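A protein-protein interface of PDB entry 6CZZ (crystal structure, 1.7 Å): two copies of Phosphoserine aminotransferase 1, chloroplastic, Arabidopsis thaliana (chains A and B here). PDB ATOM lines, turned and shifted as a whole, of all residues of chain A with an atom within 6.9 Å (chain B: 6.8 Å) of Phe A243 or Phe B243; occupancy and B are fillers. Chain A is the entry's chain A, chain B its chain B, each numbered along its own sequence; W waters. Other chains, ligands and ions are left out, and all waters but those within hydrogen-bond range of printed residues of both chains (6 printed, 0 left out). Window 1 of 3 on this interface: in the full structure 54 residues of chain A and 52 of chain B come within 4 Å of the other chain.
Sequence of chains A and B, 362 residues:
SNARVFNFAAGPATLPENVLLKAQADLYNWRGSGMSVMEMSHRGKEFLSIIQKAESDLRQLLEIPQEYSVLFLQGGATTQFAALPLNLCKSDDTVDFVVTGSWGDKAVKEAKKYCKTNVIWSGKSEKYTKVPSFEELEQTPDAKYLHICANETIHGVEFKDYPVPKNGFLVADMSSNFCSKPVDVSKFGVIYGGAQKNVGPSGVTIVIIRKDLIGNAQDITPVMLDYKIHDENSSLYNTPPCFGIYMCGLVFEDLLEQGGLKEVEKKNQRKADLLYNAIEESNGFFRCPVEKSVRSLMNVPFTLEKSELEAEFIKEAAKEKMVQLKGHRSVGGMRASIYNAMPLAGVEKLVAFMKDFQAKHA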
ATOM      1  N   ALA A  23     -16.600  10.983 -16.820  1.00  0.00           N
ATOM      2  CA  ALA A  23     -18.030  10.802 -17.031  1.00  0.00           C
ATOM      3  C   ALA A  23     -18.799  12.002 -16.527  1.00  0.00           C
ATOM      4  O   ALA A  23     -19.733  12.502 -17.190  1.00  0.00           O
ATOM      5  CB  ALA A  23     -18.503   9.538 -16.319  1.00  0.00           C
ATOM      6  N   GLN A  24     -18.387  12.517 -15.372  1.00  0.00           N
ATOM      7  CA  GLN A  24     -19.043  13.686 -14.803  1.00  0.00           C
ATOM      8  C   GLN A  24     -18.938  14.909 -15.713  1.00  0.00           C
ATOM      9  O   GLN A  24     -19.925  15.616 -15.940  1.00  0.00           O
ATOM     10  CB  GLN A  24     -18.429  13.983 -13.448  1.00  0.00           C
ATOM     11  CG  GLN A  24     -19.125  15.150 -12.737  1.00  0.00           C
ATOM     12  CD  GLN A  24     -18.422  15.558 -11.473  1.00  0.00           C
ATOM     13  OE1 GLN A  24     -17.224  15.896 -11.505  1.00  0.00           O
ATOM     14  NE2 GLN A  24     -19.156  15.555 -10.343  1.00  0.00           N
ATOM     15  N   LEU A  27     -21.251  14.463 -18.798  1.00  0.00           N
ATOM     16  CA  LEU A  27     -22.603  13.917 -18.583  1.00  0.00           C
ATOM     17  C   LEU A  27     -23.688  14.773 -19.230  1.00  0.00           C
ATOM     18  O   LEU A  27     -24.612  14.248 -19.855  1.00  0.00           O
ATOM     19  CB  LEU A  27     -22.891  13.787 -17.075  1.00  0.00           C
ATOM     20  CG  LEU A  27     -24.017  12.822 -16.692  1.00  0.00           C
ATOM     21  CD1 LEU A  27     -23.585  11.394 -17.044  1.00  0.00           C
ATOM     22  CD2 LEU A  27     -24.330  12.873 -15.241  1.00  0.00           C
ATOM     23  N   SER A  36     -26.411  14.304 -23.756  1.00  0.00           N
ATOM     24  CA  SER A  36     -25.744  13.333 -22.912  1.00  0.00           C
ATOM     25  C   SER A  36     -25.635  12.000 -23.638  1.00  0.00           C
ATOM     26  O   SER A  36     -26.446  11.700 -24.506  1.00  0.00           O
ATOM     27  CB  SER A  36     -26.578  13.137 -21.634  1.00  0.00           C
ATOM     28  OG  SER A  36     -25.984  12.183 -20.780  1.00  0.00           O
ATOM     29  N   VAL A  37     -24.637  11.188 -23.273  1.00  0.00           N
ATOM     30  CA  VAL A  37     -24.658   9.787 -23.709  1.00  0.00           C
ATOM     31  C   VAL A  37     -26.006   9.197 -23.355  1.00  0.00           C
ATOM     32  O   VAL A  37     -26.512   8.300 -24.053  1.00  0.00           O
ATOM     33  CB  VAL A  37     -23.495   8.978 -23.070  1.00  0.00           C
ATOM     34  CG1 VAL A  37     -23.582   7.428 -23.313  1.00  0.00           C
ATOM     35  CG2 VAL A  37     -22.177   9.444 -23.635  1.00  0.00           C
ATOM     36  N   MET A  38     -26.611   9.673 -22.260  1.00  0.00           N
ATOM     37  CA  MET A  38     -27.826   9.044 -21.782  1.00  0.00           C
ATOM     38  C   MET A  38     -29.018   9.369 -22.670  1.00  0.00           C
ATOM     39  O   MET A  38     -30.045   8.699 -22.536  1.00  0.00           O
ATOM     40  CB  MET A  38     -28.098   9.452 -20.328  1.00  0.00           C
ATOM     41  CG  MET A  38     -27.294   8.586 -19.364  1.00  0.00           C
ATOM     42  SD  MET A  38     -27.723   8.917 -17.612  1.00  0.00           S
ATOM     43  CE  MET A  38     -27.269  10.568 -17.433  1.00  0.00           C
ATOM     44  N   PHE A  47     -23.292   7.209 -30.623  1.00  0.00           N
ATOM     45  CA  PHE A  47     -23.258   5.990 -29.833  1.00  0.00           C
ATOM     46  C   PHE A  47     -22.541   4.880 -30.591  1.00  0.00           C
ATOM     47  O   PHE A  47     -21.804   4.104 -29.982  1.00  0.00           O
ATOM     48  CB  PHE A  47     -24.651   5.514 -29.380  1.00  0.00           C
ATOM     49  CG  PHE A  47     -24.539   4.277 -28.514  1.00  0.00           C
ATOM     50  CD1 PHE A  47     -24.104   4.396 -27.214  1.00  0.00           C
ATOM     51  CD2 PHE A  47     -24.701   3.007 -29.039  1.00  0.00           C
ATOM     52  CE1 PHE A  47     -23.896   3.285 -26.422  1.00  0.00           C
ATOM     53  CE2 PHE A  47     -24.508   1.888 -28.266  1.00  0.00           C
ATOM     54  CZ  PHE A  47     -24.095   2.002 -26.951  1.00  0.00           C
ATOM     55  N   PRO A 201     -20.121  -0.209 -14.361  1.00  0.00           N
ATOM     56  CA  PRO A 201     -21.279  -0.242 -13.464  1.00  0.00           C
ATOM     57  C   PRO A 201     -22.110  -1.460 -13.840  1.00  0.00           C
ATOM     58  O   PRO A 201     -21.840  -2.145 -14.816  1.00  0.00           O
ATOM     59  CB  PRO A 201     -22.030   1.059 -13.796  1.00  0.00           C
ATOM     60  CG  PRO A 201     -21.820   1.158 -15.327  1.00  0.00           C
ATOM     61  CD  PRO A 201     -20.386   0.590 -15.573  1.00  0.00           C
ATOM     62  N   SER A 202     -23.074  -1.785 -12.989  1.00  0.00           N
ATOM     63  CA  SER A 202     -23.892  -2.919 -13.374  1.00  0.00           C
ATOM     64  C   SER A 202     -24.886  -2.504 -14.451  1.00  0.00           C
ATOM     65  O   SER A 202     -25.182  -1.331 -14.668  1.00  0.00           O
ATOM     66  CB  SER A 202     -24.635  -3.533 -12.182  1.00  0.00           C
ATOM     67  OG  SER A 202     -25.515  -2.596 -11.613  1.00  0.00           O
ATOM     68  N   VAL A 204     -24.445  -4.110 -17.590  1.00  0.00           N
ATOM     69  CA  VAL A 204     -23.752  -4.678 -18.754  1.00  0.00           C
ATOM     70  C   VAL A 204     -23.124  -6.024 -18.389  1.00  0.00           C
ATOM     71  O   VAL A 204     -22.353  -6.123 -17.414  1.00  0.00           O
ATOM     72  CB  VAL A 204     -22.652  -3.731 -19.271  1.00  0.00           C
ATOM     73  CG1 VAL A 204     -21.960  -4.309 -20.525  1.00  0.00           C
ATOM     74  CG2 VAL A 204     -23.260  -2.327 -19.546  1.00  0.00           C
ATOM     75  N   PRO A 240     -29.703  -1.125 -26.287  1.00  0.00           N
ATOM     76  CA  PRO A 240     -28.655  -1.657 -25.398  1.00  0.00           C
ATOM     77  C   PRO A 240     -28.536  -0.817 -24.142  1.00  0.00           C
ATOM     78  O   PRO A 240     -29.144   0.263 -24.042  1.00  0.00           O
ATOM     79  CB  PRO A 240     -27.378  -1.545 -26.255  1.00  0.00           C
ATOM     80  CG  PRO A 240     -27.660  -0.396 -27.164  1.00  0.00           C
ATOM     81  CD  PRO A 240     -29.143  -0.441 -27.456  1.00  0.00           C
ATOM     82  N   PRO A 241     -27.725  -1.264 -23.150  1.00  0.00           N
ATOM     83  CA  PRO A 241     -27.457  -0.442 -21.944  1.00  0.00           C
ATOM     84  C   PRO A 241     -26.405   0.610 -22.294  1.00  0.00           C
ATOM     85  O   PRO A 241     -25.199   0.469 -21.990  1.00  0.00           O
ATOM     86  CB  PRO A 241     -26.968  -1.484 -20.935  1.00  0.00           C
ATOM     87  CG  PRO A 241     -26.254  -2.586 -21.843  1.00  0.00           C
ATOM     88  CD  PRO A 241     -27.248  -2.652 -22.996  1.00  0.00           C
ATOM     89  N   CYS A 242     -26.853   1.650 -23.016  1.00  0.00           N
ATOM     90  CA  CYS A 242     -25.912   2.577 -23.669  1.00  0.00           C
ATOM     91  C   CYS A 242     -24.938   3.174 -22.663  1.00  0.00           C
ATOM     92  O   CYS A 242     -23.715   3.206 -22.896  1.00  0.00           O
ATOM     93  CB  CYS A 242     -26.655   3.702 -24.378  1.00  0.00           C
ATOM     94  SG  CYS A 242     -27.633   3.151 -25.817  1.00  0.00           S
ATOM     95  N   PHE A 243     -25.464   3.734 -21.573  1.00  0.00           N
ATOM     96  CA  PHE A 243     -24.571   4.433 -20.654  1.00  0.00           C
ATOM     97  C   PHE A 243     -23.597   3.476 -19.958  1.00  0.00           C
ATOM     98  O   PHE A 243     -22.425   3.831 -19.752  1.00  0.00           O
ATOM     99  CB  PHE A 243     -25.386   5.241 -19.618  1.00  0.00           C
ATOM    100  CG  PHE A 243     -24.504   6.164 -18.771  1.00  0.00           C
ATOM    101  CD1 PHE A 243     -24.060   7.375 -19.301  1.00  0.00           C
ATOM    102  CD2 PHE A 243     -24.135   5.800 -17.490  1.00  0.00           C
ATOM    103  CE1 PHE A 243     -23.254   8.185 -18.560  1.00  0.00           C
ATOM    104  CE2 PHE A 243     -23.343   6.623 -16.717  1.00  0.00           C
ATOM    105  CZ  PHE A 243     -22.912   7.792 -17.236  1.00  0.00           C
ATOM    106  N   GLY A 244     -24.007   2.236 -19.645  1.00  0.00           N
ATOM    107  CA  GLY A 244     -23.070   1.277 -19.040  1.00  0.00           C
ATOM    108  C   GLY A 244     -21.996   0.856 -20.024  1.00  0.00           C
ATOM    109  O   GLY A 244     -20.835   0.662 -19.649  1.00  0.00           O
ATOM    110  N   ILE A 245     -22.372   0.703 -21.300  1.00  0.00           N
ATOM    111  CA  ILE A 245     -21.385   0.413 -22.342  1.00  0.00           C
ATOM    112  C   ILE A 245     -20.380   1.549 -22.453  1.00  0.00           C
ATOM    113  O   ILE A 245     -19.163   1.317 -22.485  1.00  0.00           O
ATOM    114  CB  ILE A 245     -22.075   0.108 -23.693  1.00  0.00           C
ATOM    115  CG1 ILE A 245     -22.773  -1.285 -23.584  1.00  0.00           C
ATOM    116  CG2 ILE A 245     -21.027   0.006 -24.813  1.00  0.00           C
ATOM    117  CD1 ILE A 245     -23.765  -1.645 -24.730  1.00  0.00           C
ATOM    118  N   TYR A 246     -20.873   2.788 -22.444  1.00  0.00           N
ATOM    119  CA  TYR A 246     -19.980   3.944 -22.482  1.00  0.00           C
ATOM    120  C   TYR A 246     -19.011   3.930 -21.302  1.00  0.00           C
ATOM    121  O   TYR A 246     -17.805   4.178 -21.469  1.00  0.00           O
ATOM    122  CB  TYR A 246     -20.831   5.210 -22.490  1.00  0.00           C
ATOM    123  CG  TYR A 246     -20.144   6.448 -21.952  1.00  0.00           C
ATOM    124  CD1 TYR A 246     -19.236   7.151 -22.701  1.00  0.00           C
ATOM    125  CD2 TYR A 246     -20.476   6.920 -20.687  1.00  0.00           C
ATOM    126  CE1 TYR A 246     -18.663   8.372 -22.208  1.00  0.00           C
ATOM    127  CE2 TYR A 246     -19.886   8.090 -20.187  1.00  0.00           C
ATOM    128  CZ  TYR A 246     -18.971   8.779 -20.953  1.00  0.00           C
ATOM    129  OH  TYR A 246     -18.416   9.946 -20.420  1.00  0.00           O
ATOM    130  N   MET A 247     -19.535   3.688 -20.095  1.00  0.00           N
ATOM    131  CA  MET A 247     -18.663   3.598 -18.915  1.00  0.00           C
ATOM    132  C   MET A 247     -17.639   2.476 -19.033  1.00  0.00           C
ATOM    133  O   MET A 247     -16.463   2.643 -18.651  1.00  0.00           O
ATOM    134  CB  MET A 247     -19.501   3.409 -17.645  1.00  0.00           C
ATOM    135  CG  MET A 247     -20.340   4.554 -17.230  1.00  0.00           C
ATOM    136  SD  MET A 247     -19.395   6.063 -16.866  1.00  0.00           S
ATOM    137  CE  MET A 247     -18.170   5.506 -15.723  1.00  0.00           C
ATOM    138  N   CYS A 248     -18.067   1.301 -19.493  1.00  0.00           N
ATOM    139  CA  CYS A 248     -17.120   0.235 -19.750  1.00  0.00           C
ATOM    140  C   CYS A 248     -16.029   0.721 -20.681  1.00  0.00           C
ATOM    141  O   CYS A 248     -14.851   0.393 -20.490  1.00  0.00           O
ATOM    142  CB  CYS A 248     -17.834  -0.971 -20.363  1.00  0.00           C
ATOM    143  SG  CYS A 248     -18.809  -1.876 -19.120  1.00  0.00           S
ATOM    144  N   GLY A 249     -16.421   1.474 -21.722  1.00  0.00           N
ATOM    145  CA  GLY A 249     -15.438   1.976 -22.659  1.00  0.00           C
ATOM    146  C   GLY A 249     -14.432   2.899 -21.997  1.00  0.00           C
ATOM    147  O   GLY A 249     -13.239   2.885 -22.335  1.00  0.00           O
ATOM    148  N   ALA B  23     -27.603  14.550 -11.601  1.00  0.00           N
ATOM    149  CA  ALA B  23     -26.754  13.375 -11.756  1.00  0.00           C
ATOM    150  C   ALA B  23     -25.291  13.782 -11.883  1.00  0.00           C
ATOM    151  O   ALA B  23     -24.412  13.161 -11.269  1.00  0.00           O
ATOM    152  CB  ALA B  23     -27.205  12.545 -12.965  1.00  0.00           C
ATOM    153  N   LEU B  27     -22.245  12.648  -9.118  1.00  0.00           N
ATOM    154  CA  LEU B  27     -21.725  11.454  -9.772  1.00  0.00           C
ATOM    155  C   LEU B  27     -20.482  10.908  -9.068  1.00  0.00           C
ATOM    156  O   LEU B  27     -20.261   9.686  -9.072  1.00  0.00           O
ATOM    157  CB  LEU B  27     -21.416  11.742 -11.249  1.00  0.00           C
ATOM    158  CG  LEU B  27     -21.324  10.457 -12.086  1.00  0.00           C
ATOM    159  CD1 LEU B  27     -22.773   9.919 -12.315  1.00  0.00           C
ATOM    160  CD2 LEU B  27     -20.608  10.689 -13.396  1.00  0.00           C
ATOM    161  N   SER B  36     -19.779   6.951  -5.731  1.00  0.00           N
ATOM    162  CA  SER B  36     -20.790   7.165  -6.755  1.00  0.00           C
ATOM    163  C   SER B  36     -21.920   6.158  -6.606  1.00  0.00           C
ATOM    164  O   SER B  36     -21.711   5.042  -6.146  1.00  0.00           O
ATOM    165  CB  SER B  36     -20.142   6.986  -8.139  1.00  0.00           C
ATOM    166  OG  SER B  36     -21.075   7.121  -9.183  1.00  0.00           O
ATOM    167  N   VAL B  37     -23.122   6.521  -7.075  1.00  0.00           N
ATOM    168  CA  VAL B  37     -24.122   5.469  -7.233  1.00  0.00           C
ATOM    169  C   VAL B  37     -23.568   4.296  -8.028  1.00  0.00           C
ATOM    170  O   VAL B  37     -23.885   3.142  -7.741  1.00  0.00           O
ATOM    171  CB  VAL B  37     -25.398   6.052  -7.876  1.00  0.00           C
ATOM    172  CG1 VAL B  37     -26.442   4.998  -8.130  1.00  0.00           C
ATOM    173  CG2 VAL B  37     -25.983   7.169  -6.992  1.00  0.00           C
ATOM    174  N   MET B  38     -22.693   4.549  -8.999  1.00  0.00           N
ATOM    175  CA  MET B  38     -22.216   3.460  -9.862  1.00  0.00           C
ATOM    176  C   MET B  38     -21.289   2.479  -9.130  1.00  0.00           C
ATOM    177  O   MET B  38     -20.969   1.416  -9.691  1.00  0.00           O
ATOM    178  CB  MET B  38     -21.486   4.054 -11.082  1.00  0.00           C
ATOM    179  CG  MET B  38     -22.438   4.575 -12.148  1.00  0.00           C
ATOM    180  SD  MET B  38     -21.515   5.192 -13.569  1.00  0.00           S
ATOM    181  CE  MET B  38     -20.687   6.598 -12.872  1.00  0.00           C
ATOM    182  N   PHE B  47     -27.935   2.320  -1.587  1.00  0.00           N
ATOM    183  CA  PHE B  47     -28.726   1.938  -2.760  1.00  0.00           C
ATOM    184  C   PHE B  47     -30.140   1.520  -2.364  1.00  0.00           C
ATOM    185  O   PHE B  47     -31.115   1.804  -3.074  1.00  0.00           O
ATOM    186  CB  PHE B  47     -28.073   0.819  -3.573  1.00  0.00           C
ATOM    187  CG  PHE B  47     -28.875   0.526  -4.814  1.00  0.00           C
ATOM    188  CD1 PHE B  47     -28.905   1.463  -5.831  1.00  0.00           C
ATOM    189  CD2 PHE B  47     -29.684  -0.605  -4.907  1.00  0.00           C
ATOM    190  CE1 PHE B  47     -29.722   1.284  -6.955  1.00  0.00           C
ATOM    191  CE2 PHE B  47     -30.476  -0.816  -6.043  1.00  0.00           C
ATOM    192  CZ  PHE B  47     -30.499   0.150  -7.061  1.00  0.00           C
ATOM    193  N   PRO B 201     -32.695   6.368 -18.695  1.00  0.00           N
ATOM    194  CA  PRO B 201     -31.755   5.833 -19.672  1.00  0.00           C
ATOM    195  C   PRO B 201     -32.092   4.380 -19.942  1.00  0.00           C
ATOM    196  O   PRO B 201     -32.871   3.742 -19.237  1.00  0.00           O
ATOM    197  CB  PRO B 201     -30.391   5.980 -18.972  1.00  0.00           C
ATOM    198  CG  PRO B 201     -30.753   5.743 -17.487  1.00  0.00           C
ATOM    199  CD  PRO B 201     -32.225   6.193 -17.307  1.00  0.00           C
ATOM    200  N   SER B 202     -31.580   3.874 -21.060  1.00  0.00           N
ATOM    201  CA  SER B 202     -31.824   2.472 -21.353  1.00  0.00           C
ATOM    202  C   SER B 202     -31.048   1.589 -20.376  1.00  0.00           C
ATOM    203  O   SER B 202     -30.023   1.982 -19.821  1.00  0.00           O
ATOM    204  CB  SER B 202     -31.457   2.148 -22.807  1.00  0.00           C
ATOM    205  OG  SER B 202     -30.184   2.657 -23.131  1.00  0.00           O
ATOM    206  N   VAL B 204     -33.029  -0.213 -17.909  1.00  0.00           N
ATOM    207  CA  VAL B 204     -34.087  -0.496 -16.921  1.00  0.00           C
ATOM    208  C   VAL B 204     -35.418  -0.720 -17.627  1.00  0.00           C
ATOM    209  O   VAL B 204     -35.791   0.050 -18.523  1.00  0.00           O
ATOM    210  CB  VAL B 204     -34.270   0.644 -15.906  1.00  0.00           C
ATOM    211  CG1 VAL B 204     -35.370   0.296 -14.881  1.00  0.00           C
ATOM    212  CG2 VAL B 204     -32.973   0.941 -15.225  1.00  0.00           C
ATOM    213  N   PRO B 240     -28.837  -5.528  -9.732  1.00  0.00           N
ATOM    214  CA  PRO B 240     -29.775  -4.768 -10.565  1.00  0.00           C
ATOM    215  C   PRO B 240     -29.037  -3.703 -11.346  1.00  0.00           C
ATOM    216  O   PRO B 240     -27.845  -3.452 -11.085  1.00  0.00           O
ATOM    217  CB  PRO B 240     -30.733  -4.146  -9.536  1.00  0.00           C
ATOM    218  CG  PRO B 240     -29.866  -4.018  -8.321  1.00  0.00           C
ATOM    219  CD  PRO B 240     -28.922  -5.157  -8.303  1.00  0.00           C
ATOM    220  N   PRO B 241     -29.684  -3.072 -12.303  1.00  0.00           N
ATOM    221  CA  PRO B 241     -29.088  -1.897 -13.004  1.00  0.00           C
ATOM    222  C   PRO B 241     -29.177  -0.671 -12.078  1.00  0.00           C
ATOM    223  O   PRO B 241     -30.032   0.222 -12.239  1.00  0.00           O
ATOM    224  CB  PRO B 241     -29.966  -1.765 -14.249  1.00  0.00           C
ATOM    225  CG  PRO B 241     -31.291  -2.298 -13.785  1.00  0.00           C
ATOM    226  CD  PRO B 241     -30.975  -3.453 -12.885  1.00  0.00           C
ATOM    227  N   CYS B 242     -28.201  -0.576 -11.160  1.00  0.00           N
ATOM    228  CA  CYS B 242     -28.270   0.403 -10.060  1.00  0.00           C
ATOM    229  C   CYS B 242     -28.318   1.836 -10.567  1.00  0.00           C
ATOM    230  O   CYS B 242     -29.198   2.604 -10.171  1.00  0.00           O
ATOM    231  CB  CYS B 242     -27.075   0.242  -9.124  1.00  0.00           C
ATOM    232  SG  CYS B 242     -27.115  -1.303  -8.239  1.00  0.00           S
ATOM    233  N   PHE B 243     -27.405   2.204 -11.479  1.00  0.00           N
ATOM    234  CA  PHE B 243     -27.390   3.583 -11.951  1.00  0.00           C
ATOM    235  C   PHE B 243     -28.662   3.939 -12.734  1.00  0.00           C
ATOM    236  O   PHE B 243     -29.193   5.043 -12.589  1.00  0.00           O
ATOM    237  CB  PHE B 243     -26.141   3.874 -12.808  1.00  0.00           C
ATOM    238  CG  PHE B 243     -25.971   5.348 -13.054  1.00  0.00           C
ATOM    239  CD1 PHE B 243     -25.581   6.174 -11.995  1.00  0.00           C
ATOM    240  CD2 PHE B 243     -26.183   5.901 -14.324  1.00  0.00           C
ATOM    241  CE1 PHE B 243     -25.434   7.548 -12.185  1.00  0.00           C
ATOM    242  CE2 PHE B 243     -26.036   7.243 -14.546  1.00  0.00           C
ATOM    243  CZ  PHE B 243     -25.680   8.088 -13.500  1.00  0.00           C
ATOM    244  N   GLY B 244     -29.152   3.046 -13.592  1.00  0.00           N
ATOM    245  CA  GLY B 244     -30.378   3.347 -14.318  1.00  0.00           C
ATOM    246  C   GLY B 244     -31.585   3.498 -13.386  1.00  0.00           C
ATOM    247  O   GLY B 244     -32.437   4.360 -13.594  1.00  0.00           O
ATOM    248  N   ILE B 245     -31.660   2.668 -12.346  1.00  0.00           N
ATOM    249  CA  ILE B 245     -32.741   2.791 -11.351  1.00  0.00           C
ATOM    250  C   ILE B 245     -32.645   4.135 -10.610  1.00  0.00           C
ATOM    251  O   ILE B 245     -33.648   4.841 -10.430  1.00  0.00           O
ATOM    252  CB  ILE B 245     -32.723   1.591 -10.384  1.00  0.00           C
ATOM    253  CG1 ILE B 245     -33.121   0.292 -11.129  1.00  0.00           C
ATOM    254  CG2 ILE B 245     -33.610   1.845  -9.184  1.00  0.00           C
ATOM    255  CD1 ILE B 245     -32.904  -1.004 -10.292  1.00  0.00           C
ATOM    256  N   TYR B 246     -31.430   4.526 -10.235  1.00  0.00           N
ATOM    257  CA  TYR B 246     -31.202   5.857  -9.685  1.00  0.00           C
ATOM    258  C   TYR B 246     -31.678   6.968 -10.628  1.00  0.00           C
ATOM    259  O   TYR B 246     -32.402   7.880 -10.201  1.00  0.00           O
ATOM    260  CB  TYR B 246     -29.729   5.991  -9.330  1.00  0.00           C
ATOM    261  CG  TYR B 246     -29.208   7.413  -9.228  1.00  0.00           C
ATOM    262  CD1 TYR B 246     -29.490   8.194  -8.114  1.00  0.00           C
ATOM    263  CD2 TYR B 246     -28.430   7.938 -10.249  1.00  0.00           C
ATOM    264  CE1 TYR B 246     -29.003   9.492  -8.015  1.00  0.00           C
ATOM    265  CE2 TYR B 246     -27.942   9.259 -10.159  1.00  0.00           C
ATOM    266  CZ  TYR B 246     -28.223   9.990  -9.037  1.00  0.00           C
ATOM    267  OH  TYR B 246     -27.770  11.273  -8.949  1.00  0.00           O
ATOM    268  N   MET B 247     -31.279   6.903 -11.913  1.00  0.00           N
ATOM    269  CA  MET B 247     -31.728   7.887 -12.888  1.00  0.00           C
ATOM    270  C   MET B 247     -33.249   7.908 -13.020  1.00  0.00           C
ATOM    271  O   MET B 247     -33.852   8.986 -13.107  1.00  0.00           O
ATOM    272  CB  MET B 247     -31.063   7.623 -14.251  1.00  0.00           C
ATOM    273  CG  MET B 247     -29.536   7.891 -14.273  1.00  0.00           C
ATOM    274  SD  MET B 247     -29.131   9.614 -13.867  1.00  0.00           S
ATOM    275  CE  MET B 247     -30.130  10.504 -15.030  1.00  0.00           C
ATOM    276  N   CYS B 248     -33.896   6.732 -13.054  1.00  0.00           N
ATOM    277  CA  CYS B 248     -35.361   6.726 -13.089  1.00  0.00           C
ATOM    278  C   CYS B 248     -35.931   7.429 -11.868  1.00  0.00           C
ATOM    279  O   CYS B 248     -36.936   8.130 -11.959  1.00  0.00           O
ATOM    280  CB  CYS B 248     -35.896   5.314 -13.108  1.00  0.00           C
ATOM    281  SG  CYS B 248     -35.595   4.518 -14.733  1.00  0.00           S
ATOM    282  N   GLY B 249     -35.329   7.200 -10.701  1.00  0.00           N
ATOM    283  CA  GLY B 249     -35.765   7.874  -9.509  1.00  0.00           C
ATOM    284  C   GLY B 249     -35.683   9.390  -9.599  1.00  0.00           C
ATOM    285  O   GLY B 249     -36.582  10.094  -9.111  1.00  0.00           O
HETATM  286  O   HOH W   1     -28.303   4.005 -20.979  1.00  0.00           O
HETATM  287  O   HOH W   2     -27.523   0.740 -14.698  1.00  0.00           O
HETATM  288  O   HOH W   3     -23.266  -0.100 -10.483  1.00  0.00           O
HETATM  289  O   HOH W   4     -27.000   1.610 -19.247  1.00  0.00           O
HETATM  290  O   HOH W   5     -25.200   0.464 -12.442  1.00  0.00           O
HETATM  291  O   HOH W   6     -29.782   5.741 -22.727  1.00  0.00           O
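Water W5 lies within hydrogen-bond range of the backbone carbonyl oxygen (O) of Ser A202, the backbone NH (N) of Phe B243 and the backbone NH (N) of Cys B242. Water W6 lies within hydrogen-bond range of O of Met A38 (3.0 Å) and N of Ser B202 (3.1 Å). Water W2 bridges N of Gly B244 and O of Ser A202. Water W4 lies within hydrogen-bond range of N of Gly A244, O of Ser B202 and O of Pro A241.
Of the printed residues of chain B, Ala A23 touches Leu B27 (3.8 Å). Printed residues of chain B within 4 Å of Leu A27: Ala B23 (3.6 Å). Val A37 touches none of the printed residues of chain B. Of the printed residues of chain B, Met A38 touches Phe B243 (3.9 Å) and Met B247 (3.7 Å). Printed residues of chain B within 4 Å of Pro A240: Ser B202. Of the printed residues of chain B, Cys A242 touches Ser B202 (3.5 Å). Of chain B, only Met B38 (3.9 Å) and Phe B243 (3.5 Å) come within 4 Å of Phe A243. Ile A245 touches none of the printed residues of chain B. Of chain A, only Met A38 (3.9 Å) and Phe A243 (3.5 Å) come within 4 Å of Phe B243. The nearest printed residue of chain B that does not touch Phe A243 is Ser B202 (5.1 Å). The nearest printed residue of chain A that does not touch Ser B202 is Pro A241 (4.1 Å).
Met A38 touches Phe B243, and with the chains exchanged Phe A243 touches Met B38. Met A38 touches Met B247, and with the chains exchanged Met A247 touches Met B38. Ser A202 touches Cys B242, and with the chains exchanged Cys A242 touches Ser B202. Phe B243 touches its own counterpart, Phe A243. 19 positions are printed for both chains. Of the 14 pairs that touch across the chains among the printed residues, 11 have their exchanged pair printed and touching as well.
Ala A23 touches Leu B27. Leu B27 touches Gln A24. Ala B23 touches Leu A27 (C to CD2, 3.6 Å). Met A38 touches Phe B243. CE of Met A38 touches CE of Met B247, at 3.7 Å. CB of Pro A201 touches CG of Met B38, 3.9 Å away. Ser A202 touches Pro B241 (OG to CA, 3.9 Å). Phe A243 touches Met B38. CE2 of Phe A243 touches CE2 of Phe B243, at 3.5 Å. CG of Met A247 touches SD of Met B38, 3.9 Å away.
The side-chain hydroxyl (OG) of Ser B202 lies within hydrogen-bond range of the backbone carbonyl oxygen (O) of Pro A240, at 2.8 Å. The side-chain hydroxyl (OG) of Ser A202 lies within hydrogen-bond range of the backbone NH (N) of Cys B242. O of Pro B240 sits at hydrogen-bond distance from OG of Ser A202 (2.5 Å). N of Cys A242 sits at hydrogen-bond distance from OG of Ser B202, at 3.5 Å.
Of the 19 printed residues of chain B, 9 touch a printed residue of chain A. Hydrophobic or aromatic side chains of chain B within 4 Å of the printed part of chain A: Ala B23, Leu B27, Met B38, Phe B243 and Met B247. Along chain B the printed residues that touch a printed residue of chain A span positions 23 to 247. Of the 20 printed residues of chain A, 10 touch a printed residue of chain B. Among the printed residues, 14 pairs touch across the chains.
The side-chain hydroxyl (OG) of Ser B36 sits close to the backbone NH (N) of Met B38 (3.0 Å). The backbone carbonyl oxygen (O) of Leu A27 is in hydrogen-bond range of the side-chain hydroxyl (OG) of Ser A36, at 2.6 Å. The side-chain hydroxyl of Ser A36 lies close to the backbone NH of Met A38. O of Pro A240 is in hydrogen-bond range of SG of Cys A242, 3.7 Å away. The backbone carbonyl oxygen of Leu B27 sits at hydrogen-bond distance from the side-chain hydroxyl of Ser B36, at 2.7 Å. SG of Cys B242 sits at hydrogen-bond distance from O of Pro B240 (3.6 Å).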
